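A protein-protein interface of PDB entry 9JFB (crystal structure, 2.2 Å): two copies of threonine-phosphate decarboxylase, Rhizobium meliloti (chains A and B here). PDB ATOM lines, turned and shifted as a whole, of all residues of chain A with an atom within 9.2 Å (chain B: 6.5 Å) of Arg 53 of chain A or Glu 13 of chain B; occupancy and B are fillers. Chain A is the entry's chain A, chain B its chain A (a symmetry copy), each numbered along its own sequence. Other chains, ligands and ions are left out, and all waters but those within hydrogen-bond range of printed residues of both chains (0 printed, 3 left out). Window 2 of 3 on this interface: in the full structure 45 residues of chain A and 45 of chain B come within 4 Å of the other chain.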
ATOM      1  N   ARG A  49      -0.082  -1.602   4.249  1.00  0.00           N
ATOM      2  CA  ARG A  49       0.088  -3.047   4.117  1.00  0.00           C
ATOM      3  C   ARG A  49      -1.246  -3.766   3.914  1.00  0.00           C
ATOM      4  O   ARG A  49      -2.275  -3.381   4.479  1.00  0.00           O
ATOM      5  CB  ARG A  49       0.763  -3.628   5.370  1.00  0.00           C
ATOM      6  CG  ARG A  49       2.145  -3.048   5.702  1.00  0.00           C
ATOM      7  CD  ARG A  49       2.725  -3.691   6.975  1.00  0.00           C
ATOM      8  NE  ARG A  49       2.681  -5.148   6.925  1.00  0.00           N
ATOM      9  CZ  ARG A  49       3.506  -5.896   6.202  1.00  0.00           C
ATOM     10  NH1 ARG A  49       4.483  -5.356   5.486  1.00  0.00           N
ATOM     11  NH2 ARG A  49       3.348  -7.217   6.195  1.00  0.00           N
ATOM     12  N   LEU A  50      -1.209  -4.831   3.118  1.00  0.00           N
ATOM     13  CA  LEU A  50      -2.264  -5.829   3.168  1.00  0.00           C
ATOM     14  C   LEU A  50      -2.536  -6.176   4.628  1.00  0.00           C
ATOM     15  O   LEU A  50      -1.586  -6.311   5.411  1.00  0.00           O
ATOM     16  CB  LEU A  50      -1.858  -7.089   2.393  1.00  0.00           C
ATOM     17  CG  LEU A  50      -1.687  -6.897   0.887  1.00  0.00           C
ATOM     18  CD1 LEU A  50      -0.964  -8.089   0.278  1.00  0.00           C
ATOM     19  CD2 LEU A  50      -3.048  -6.687   0.196  1.00  0.00           C
ATOM     20  N   PRO A  51      -3.799  -6.289   5.036  1.00  0.00           N
ATOM     21  CA  PRO A  51      -4.099  -6.426   6.475  1.00  0.00           C
ATOM     22  C   PRO A  51      -3.441  -7.668   7.055  1.00  0.00           C
ATOM     23  O   PRO A  51      -3.674  -8.786   6.595  1.00  0.00           O
ATOM     24  CB  PRO A  51      -5.636  -6.492   6.524  1.00  0.00           C
ATOM     25  CG  PRO A  51      -6.097  -6.564   5.077  1.00  0.00           C
ATOM     26  CD  PRO A  51      -4.997  -6.017   4.230  1.00  0.00           C
ATOM     27  N   ASP A  52      -2.573  -7.450   8.043  1.00  0.00           N
ATOM     28  CA  ASP A  52      -1.737  -8.486   8.638  1.00  0.00           C
ATOM     29  C   ASP A  52      -2.531  -9.326   9.627  1.00  0.00           C
ATOM     30  O   ASP A  52      -3.523  -8.874  10.207  1.00  0.00           O
ATOM     31  CB  ASP A  52      -0.542  -7.864   9.366  1.00  0.00           C
ATOM     32  CG  ASP A  52       0.453  -7.223   8.421  1.00  0.00           C
ATOM     33  OD1 ASP A  52       1.028  -7.947   7.574  1.00  0.00           O
ATOM     34  OD2 ASP A  52       0.654  -5.988   8.520  1.00  0.00           O
ATOM     35  N   ARG A  53      -2.067 -10.562   9.837  1.00  0.00           N
ATOM     36  CA  ARG A  53      -2.758 -11.443  10.770  1.00  0.00           C
ATOM     37  C   ARG A  53      -2.828 -10.832  12.166  1.00  0.00           C
ATOM     38  O   ARG A  53      -3.820 -11.016  12.877  1.00  0.00           O
ATOM     39  CB  ARG A  53      -2.080 -12.806  10.825  1.00  0.00           C
ATOM     40  CG  ARG A  53      -2.836 -13.794  11.698  1.00  0.00           C
ATOM     41  CD  ARG A  53      -1.972 -14.972  12.092  1.00  0.00           C
ATOM     42  NE  ARG A  53      -1.986 -16.028  11.090  1.00  0.00           N
ATOM     43  CZ  ARG A  53      -2.932 -16.951  10.999  1.00  0.00           C
ATOM     44  NH1 ARG A  53      -3.985 -16.942  11.802  1.00  0.00           N
ATOM     45  NH2 ARG A  53      -2.815 -17.908  10.083  1.00  0.00           N
ATOM     46  N   GLN A  54      -1.784 -10.108  12.577  1.00  0.00           N
ATOM     47  CA  GLN A  54      -1.802  -9.470  13.894  1.00  0.00           C
ATOM     48  C   GLN A  54      -2.890  -8.399  13.993  1.00  0.00           C
ATOM     49  O   GLN A  54      -3.539  -8.265  15.035  1.00  0.00           O
ATOM     50  CB  GLN A  54      -0.437  -8.856  14.198  1.00  0.00           C
ATOM     51  CG  GLN A  54      -0.310  -8.334  15.617  1.00  0.00           C
ATOM     52  CD  GLN A  54      -0.371  -9.474  16.623  1.00  0.00           C
ATOM     53  OE1 GLN A  54       0.399 -10.430  16.534  1.00  0.00           O
ATOM     54  NE2 GLN A  54      -1.310  -9.396  17.561  1.00  0.00           N
ATOM     55  N   THR A  55      -3.068  -7.594  12.938  1.00  0.00           N
ATOM     56  CA  THR A  55      -4.132  -6.587  12.936  1.00  0.00           C
ATOM     57  C   THR A  55      -5.502  -7.245  13.084  1.00  0.00           C
ATOM     58  O   THR A  55      -6.351  -6.802  13.878  1.00  0.00           O
ATOM     59  CB  THR A  55      -4.071  -5.776  11.637  1.00  0.00           C
ATOM     60  OG1 THR A  55      -2.730  -5.325  11.401  1.00  0.00           O
ATOM     61  CG2 THR A  55      -5.009  -4.581  11.706  1.00  0.00           C
ATOM     62  N   VAL A  56      -5.723  -8.327  12.328  1.00  0.00           N
ATOM     63  CA  VAL A  56      -6.950  -9.103  12.450  1.00  0.00           C
ATOM     64  C   VAL A  56      -7.122  -9.612  13.877  1.00  0.00           C
ATOM     65  O   VAL A  56      -8.174  -9.419  14.494  1.00  0.00           O
ATOM     66  CB  VAL A  56      -6.956 -10.259  11.434  1.00  0.00           C
ATOM     67  CG1 VAL A  56      -8.158 -11.179  11.678  1.00  0.00           C
ATOM     68  CG2 VAL A  56      -6.963  -9.715   9.993  1.00  0.00           C
ATOM     69  N   ASP A  57      -6.094 -10.282  14.416  1.00  0.00           N
ATOM     70  CA  ASP A  57      -6.225 -10.918  15.725  1.00  0.00           C
ATOM     71  C   ASP A  57      -6.508  -9.894  16.821  1.00  0.00           C
ATOM     72  O   ASP A  57      -7.278 -10.169  17.745  1.00  0.00           O
ATOM     73  CB  ASP A  57      -4.964 -11.708  16.069  1.00  0.00           C
ATOM     74  CG  ASP A  57      -4.779 -12.970  15.206  1.00  0.00           C
ATOM     75  OD1 ASP A  57      -5.757 -13.468  14.604  1.00  0.00           O
ATOM     76  OD2 ASP A  57      -3.633 -13.472  15.149  1.00  0.00           O
ATOM     77  N   ASP A  58      -5.858  -8.731  16.761  1.00  0.00           N
ATOM     78  CA  ASP A  58      -6.147  -7.669  17.720  1.00  0.00           C
ATOM     79  C   ASP A  58      -7.610  -7.254  17.644  1.00  0.00           C
ATOM     80  O   ASP A  58      -8.278  -7.093  18.676  1.00  0.00           O
ATOM     81  CB  ASP A  58      -5.235  -6.466  17.462  1.00  0.00           C
ATOM     82  CG  ASP A  58      -3.773  -6.743  17.822  1.00  0.00           C
ATOM     83  OD1 ASP A  58      -3.497  -7.812  18.403  1.00  0.00           O
ATOM     84  OD2 ASP A  58      -2.904  -5.897  17.508  1.00  0.00           O
ATOM     85  N   ALA A  59      -8.128  -7.068  16.421  1.00  0.00           N
ATOM     86  CA  ALA A  59      -9.541  -6.722  16.296  1.00  0.00           C
ATOM     87  C   ALA A  59     -10.429  -7.815  16.883  1.00  0.00           C
ATOM     88  O   ALA A  59     -11.415  -7.523  17.572  1.00  0.00           O
ATOM     89  CB  ALA A  59      -9.897  -6.458  14.833  1.00  0.00           C
ATOM     90  N   ARG A  60     -10.074  -9.082  16.653  1.00  0.00           N
ATOM     91  CA  ARG A  60     -10.899 -10.191  17.128  1.00  0.00           C
ATOM     92  C   ARG A  60     -10.910 -10.285  18.652  1.00  0.00           C
ATOM     93  O   ARG A  60     -11.964 -10.550  19.244  1.00  0.00           O
ATOM     94  CB  ARG A  60     -10.421 -11.514  16.527  1.00  0.00           C
ATOM     95  CG  ARG A  60     -10.448 -11.548  15.000  1.00  0.00           C
ATOM     96  CD  ARG A  60     -10.157 -12.949  14.501  1.00  0.00           C
ATOM     97  NE  ARG A  60     -11.246 -13.893  14.734  1.00  0.00           N
ATOM     98  CZ  ARG A  60     -11.199 -15.173  14.380  1.00  0.00           C
ATOM     99  NH1 ARG A  60     -10.120 -15.693  13.813  1.00  0.00           N
ATOM    100  NH2 ARG A  60     -12.260 -15.954  14.595  1.00  0.00           N
ATOM    101  N   SER A  61      -9.750 -10.094  19.303  1.00  0.00           N
ATOM    102  CA  SER A  61      -9.707 -10.107  20.770  1.00  0.00           C
ATOM    103  C   SER A  61     -10.505  -8.950  21.352  1.00  0.00           C
ATOM    104  O   SER A  61     -11.251  -9.125  22.331  1.00  0.00           O
ATOM    105  CB  SER A  61      -8.265 -10.029  21.288  1.00  0.00           C
ATOM    106  OG  SER A  61      -7.491 -11.098  20.808  1.00  0.00           O
ATOM    107  N   LEU A  73     -13.604 -16.084  19.644  1.00  0.00           N
ATOM    108  CA  LEU A  73     -13.047 -14.972  18.893  1.00  0.00           C
ATOM    109  C   LEU A  73     -13.933 -14.672  17.689  1.00  0.00           C
ATOM    110  O   LEU A  73     -13.965 -15.472  16.739  1.00  0.00           O
ATOM    111  CB  LEU A  73     -11.642 -15.291  18.443  1.00  0.00           C
ATOM    112  CG  LEU A  73     -10.622 -15.428  19.571  1.00  0.00           C
ATOM    113  CD1 LEU A  73      -9.327 -15.972  19.001  1.00  0.00           C
ATOM    114  CD2 LEU A  73     -10.392 -14.068  20.215  1.00  0.00           C
ATOM    115  N   PRO A  76     -14.056 -11.042  11.969  1.00  0.00           N
ATOM    116  CA  PRO A  76     -14.353  -9.785  11.274  1.00  0.00           C
ATOM    117  C   PRO A  76     -14.726 -10.070   9.832  1.00  0.00           C
ATOM    118  O   PRO A  76     -14.120 -10.918   9.178  1.00  0.00           O
ATOM    119  CB  PRO A  76     -13.034  -9.000  11.354  1.00  0.00           C
ATOM    120  CG  PRO A  76     -12.101  -9.846  12.230  1.00  0.00           C
ATOM    121  CD  PRO A  76     -12.608 -11.258  12.098  1.00  0.00           C
ATOM    122  N   TRP A 228      -7.702 -11.176   3.066  1.00  0.00           N
ATOM    123  CA  TRP A 228      -7.711  -9.709   3.145  1.00  0.00           C
ATOM    124  C   TRP A 228      -9.112  -9.137   2.906  1.00  0.00           C
ATOM    125  O   TRP A 228      -9.284  -8.153   2.182  1.00  0.00           O
ATOM    126  CB  TRP A 228      -6.720  -9.095   2.146  1.00  0.00           C
ATOM    127  CG  TRP A 228      -5.366  -9.729   2.099  1.00  0.00           C
ATOM    128  CD1 TRP A 228      -4.441  -9.783   3.109  1.00  0.00           C
ATOM    129  CD2 TRP A 228      -4.768 -10.386   0.971  1.00  0.00           C
ATOM    130  NE1 TRP A 228      -3.312 -10.449   2.676  1.00  0.00           N
ATOM    131  CE2 TRP A 228      -3.484 -10.813   1.366  1.00  0.00           C
ATOM    132  CE3 TRP A 228      -5.192 -10.645  -0.337  1.00  0.00           C
ATOM    133  CZ2 TRP A 228      -2.625 -11.490   0.500  1.00  0.00           C
ATOM    134  CZ3 TRP A 228      -4.344 -11.318  -1.196  1.00  0.00           C
ATOM    135  CH2 TRP A 228      -3.070 -11.732  -0.774  1.00  0.00           C
ATOM    136  N   LEU A 235     -10.084  -2.467  10.880  1.00  0.00           N
ATOM    137  CA  LEU A 235      -9.678  -3.329  11.991  1.00  0.00           C
ATOM    138  C   LEU A 235      -8.950  -2.539  13.081  1.00  0.00           C
ATOM    139  O   LEU A 235      -9.157  -2.775  14.278  1.00  0.00           O
ATOM    140  CB  LEU A 235      -8.793  -4.461  11.451  1.00  0.00           C
ATOM    141  CG  LEU A 235      -9.432  -5.439  10.448  1.00  0.00           C
ATOM    142  CD1 LEU A 235      -8.377  -6.230   9.673  1.00  0.00           C
ATOM    143  CD2 LEU A 235     -10.362  -6.403  11.182  1.00  0.00           C
ATOM    144  N   GLY B   9       3.399 -11.123   2.246  1.00  0.00           N
ATOM    145  CA  GLY B   9       3.018 -10.164   3.263  1.00  0.00           C
ATOM    146  C   GLY B   9       2.913 -10.732   4.659  1.00  0.00           C
ATOM    147  O   GLY B   9       2.556  -9.990   5.585  1.00  0.00           O
ATOM    148  N   GLY B  10       3.222 -12.013   4.845  1.00  0.00           N
ATOM    149  CA  GLY B  10       3.022 -12.657   6.131  1.00  0.00           C
ATOM    150  C   GLY B  10       4.077 -12.345   7.173  1.00  0.00           C
ATOM    151  O   GLY B  10       4.733 -13.257   7.688  1.00  0.00           O
ATOM    152  N   ILE B  11       4.222 -11.062   7.520  1.00  0.00           N
ATOM    153  CA  ILE B  11       5.234 -10.661   8.490  1.00  0.00           C
ATOM    154  C   ILE B  11       4.899 -11.170   9.882  1.00  0.00           C
ATOM    155  O   ILE B  11       5.806 -11.510  10.647  1.00  0.00           O
ATOM    156  CB  ILE B  11       5.415  -9.137   8.482  1.00  0.00           C
ATOM    157  CG1 ILE B  11       6.180  -8.715   7.226  1.00  0.00           C
ATOM    158  CG2 ILE B  11       6.185  -8.687   9.712  1.00  0.00           C
ATOM    159  CD1 ILE B  11       7.620  -9.218   7.201  1.00  0.00           C
ATOM    160  N   THR B  12       3.610 -11.233  10.242  1.00  0.00           N
ATOM    161  CA  THR B  12       3.227 -11.753  11.554  1.00  0.00           C
ATOM    162  C   THR B  12       3.770 -13.168  11.759  1.00  0.00           C
ATOM    163  O   THR B  12       4.455 -13.455  12.749  1.00  0.00           O
ATOM    164  CB  THR B  12       1.691 -11.737  11.703  1.00  0.00           C
ATOM    165  OG1 THR B  12       1.183 -10.405  11.514  1.00  0.00           O
ATOM    166  CG2 THR B  12       1.269 -12.244  13.084  1.00  0.00           C
ATOM    167  N   GLU B  13       3.488 -14.062  10.816  1.00  0.00           N
ATOM    168  CA  GLU B  13       3.974 -15.436  10.916  1.00  0.00           C
ATOM    169  C   GLU B  13       5.506 -15.509  10.833  1.00  0.00           C
ATOM    170  O   GLU B  13       6.141 -16.280  11.570  1.00  0.00           O
ATOM    171  CB  GLU B  13       3.325 -16.279   9.819  1.00  0.00           C
ATOM    172  CG  GLU B  13       1.781 -16.301   9.863  1.00  0.00           C
ATOM    173  CD  GLU B  13       1.098 -15.132   9.116  1.00  0.00           C
ATOM    174  OE1 GLU B  13       1.668 -14.018   9.009  1.00  0.00           O
ATOM    175  OE2 GLU B  13      -0.034 -15.337   8.634  1.00  0.00           O
ATOM    176  N   ALA B  14       6.120 -14.721   9.945  1.00  0.00           N
ATOM    177  CA  ALA B  14       7.573 -14.760   9.804  1.00  0.00           C
ATOM    178  C   ALA B  14       8.259 -14.330  11.093  1.00  0.00           C
ATOM    179  O   ALA B  14       9.188 -14.991  11.560  1.00  0.00           O
ATOM    180  CB  ALA B  14       8.026 -13.870   8.649  1.00  0.00           C
ATOM    181  N   ALA B  15       7.826 -13.207  11.669  1.00  0.00           N
ATOM    182  CA  ALA B  15       8.395 -12.736  12.924  1.00  0.00           C
ATOM    183  C   ALA B  15       8.137 -13.716  14.062  1.00  0.00           C
ATOM    184  O   ALA B  15       8.978 -13.859  14.957  1.00  0.00           O
ATOM    185  CB  ALA B  15       7.835 -11.356  13.271  1.00  0.00           C
ATOM    186  N   ALA B  16       7.001 -14.415  14.045  1.00  0.00           N
ATOM    187  CA  ALA B  16       6.792 -15.438  15.062  1.00  0.00           C
ATOM    188  C   ALA B  16       7.785 -16.585  14.903  1.00  0.00           C
ATOM    189  O   ALA B  16       8.248 -17.153  15.896  1.00  0.00           O
ATOM    190  CB  ALA B  16       5.351 -15.958  15.007  1.00  0.00           C
ATOM    191  N   ARG B  17       8.120 -16.942  13.663  1.00  0.00           N
ATOM    192  CA  ARG B  17       8.945 -18.123  13.436  1.00  0.00           C
ATOM    193  C   ARG B  17      10.435 -17.818  13.555  1.00  0.00           C
ATOM    194  O   ARG B  17      11.202 -18.648  14.050  1.00  0.00           O
ATOM    195  CB  ARG B  17       8.630 -18.700  12.068  1.00  0.00           C
ATOM    196  CG  ARG B  17       9.385 -19.939  11.712  1.00  0.00           C
ATOM    197  CD  ARG B  17       8.781 -20.497  10.437  1.00  0.00           C
ATOM    198  NE  ARG B  17       9.517 -21.642   9.923  1.00  0.00           N
ATOM    199  CZ  ARG B  17       9.262 -22.222   8.760  1.00  0.00           C
ATOM    200  NH1 ARG B  17       8.298 -21.779   7.965  1.00  0.00           N
ATOM    201  NH2 ARG B  17       9.990 -23.271   8.383  1.00  0.00           N
ATOM    202  N   TYR B  18      10.852 -16.632  13.125  1.00  0.00           N
ATOM    203  CA  TYR B  18      12.251 -16.258  13.002  1.00  0.00           C
ATOM    204  C   TYR B  18      12.664 -15.156  13.963  1.00  0.00           C
ATOM    205  O   TYR B  18      13.835 -14.764  13.963  1.00  0.00           O
ATOM    206  CB  TYR B  18      12.548 -15.815  11.562  1.00  0.00           C
ATOM    207  CG  TYR B  18      12.418 -16.930  10.546  1.00  0.00           C
ATOM    208  CD1 TYR B  18      13.441 -17.858  10.371  1.00  0.00           C
ATOM    209  CD2 TYR B  18      11.276 -17.061   9.769  1.00  0.00           C
ATOM    210  CE1 TYR B  18      13.331 -18.890   9.445  1.00  0.00           C
ATOM    211  CE2 TYR B  18      11.153 -18.092   8.840  1.00  0.00           C
ATOM    212  CZ  TYR B  18      12.187 -19.003   8.682  1.00  0.00           C
ATOM    213  OH  TYR B  18      12.089 -20.018   7.753  1.00  0.00           O
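No position is printed for both chains. Of the 7 pairs that touch across the chains among the printed residues, none has its exchanged pair printed and touching as well.
Ser 61 of chain A touches none of the printed residues of chain B. Printed residues of chain A within 4 Å of Ile 11 of chain B: Arg 49 (3.4 Å). Of the printed residues of chain A, Thr 12 of chain B touches Asp 52 (3.7 Å), Arg 53 (3.7 Å) and Gln 54 (3.2 Å). Of the printed residues of chain A, Glu 13 of chain B touches Arg 53. No residue of chain A comes within 4 Å of Ala 14 of chain B. No residue of chain A comes within 4 Å of Ala 16 of chain B.
NE of Arg 49 of chain A is in salt-bridge range of OD2 of Asp 52 of chain A (2.7 Å). NE2 of Gln 54 of chain A lies within hydrogen-bond range of OD1 of Asp 58 of chain A.
Hydrophobic or aromatic side chains of chain B within 4 Å of the printed part of chain A: Ile 11.
Arg 49 of chain A touches Ile 11 of chain B. CB of Asp 52 of chain A touches OG1 of Thr 12 of chain B (3.7 Å). Arg 53 of chain A touches Thr 12 of chain B (N to OG1, 3.7 Å).
The guanidinium group (NH2) of Arg 49 of chain A lies within hydrogen-bond range of the backbone carbonyl oxygen (O) of Gly 9 of chain B (2.9 Å). The guanidinium group of Arg 53 of chain A is in salt-bridge range of the side-chain carboxylate of Glu 13 of chain B, at 3.2 Å. N of Gln 54 of chain A lies within hydrogen-bond range of OG1 of Thr 12 of chain B (3.2 Å). The side-chain carboxylate (OD1) of Asp 52 of chain A sits close to the backbone carbonyl oxygen (O) of Gly 9 of chain B, at 3.2 Å.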
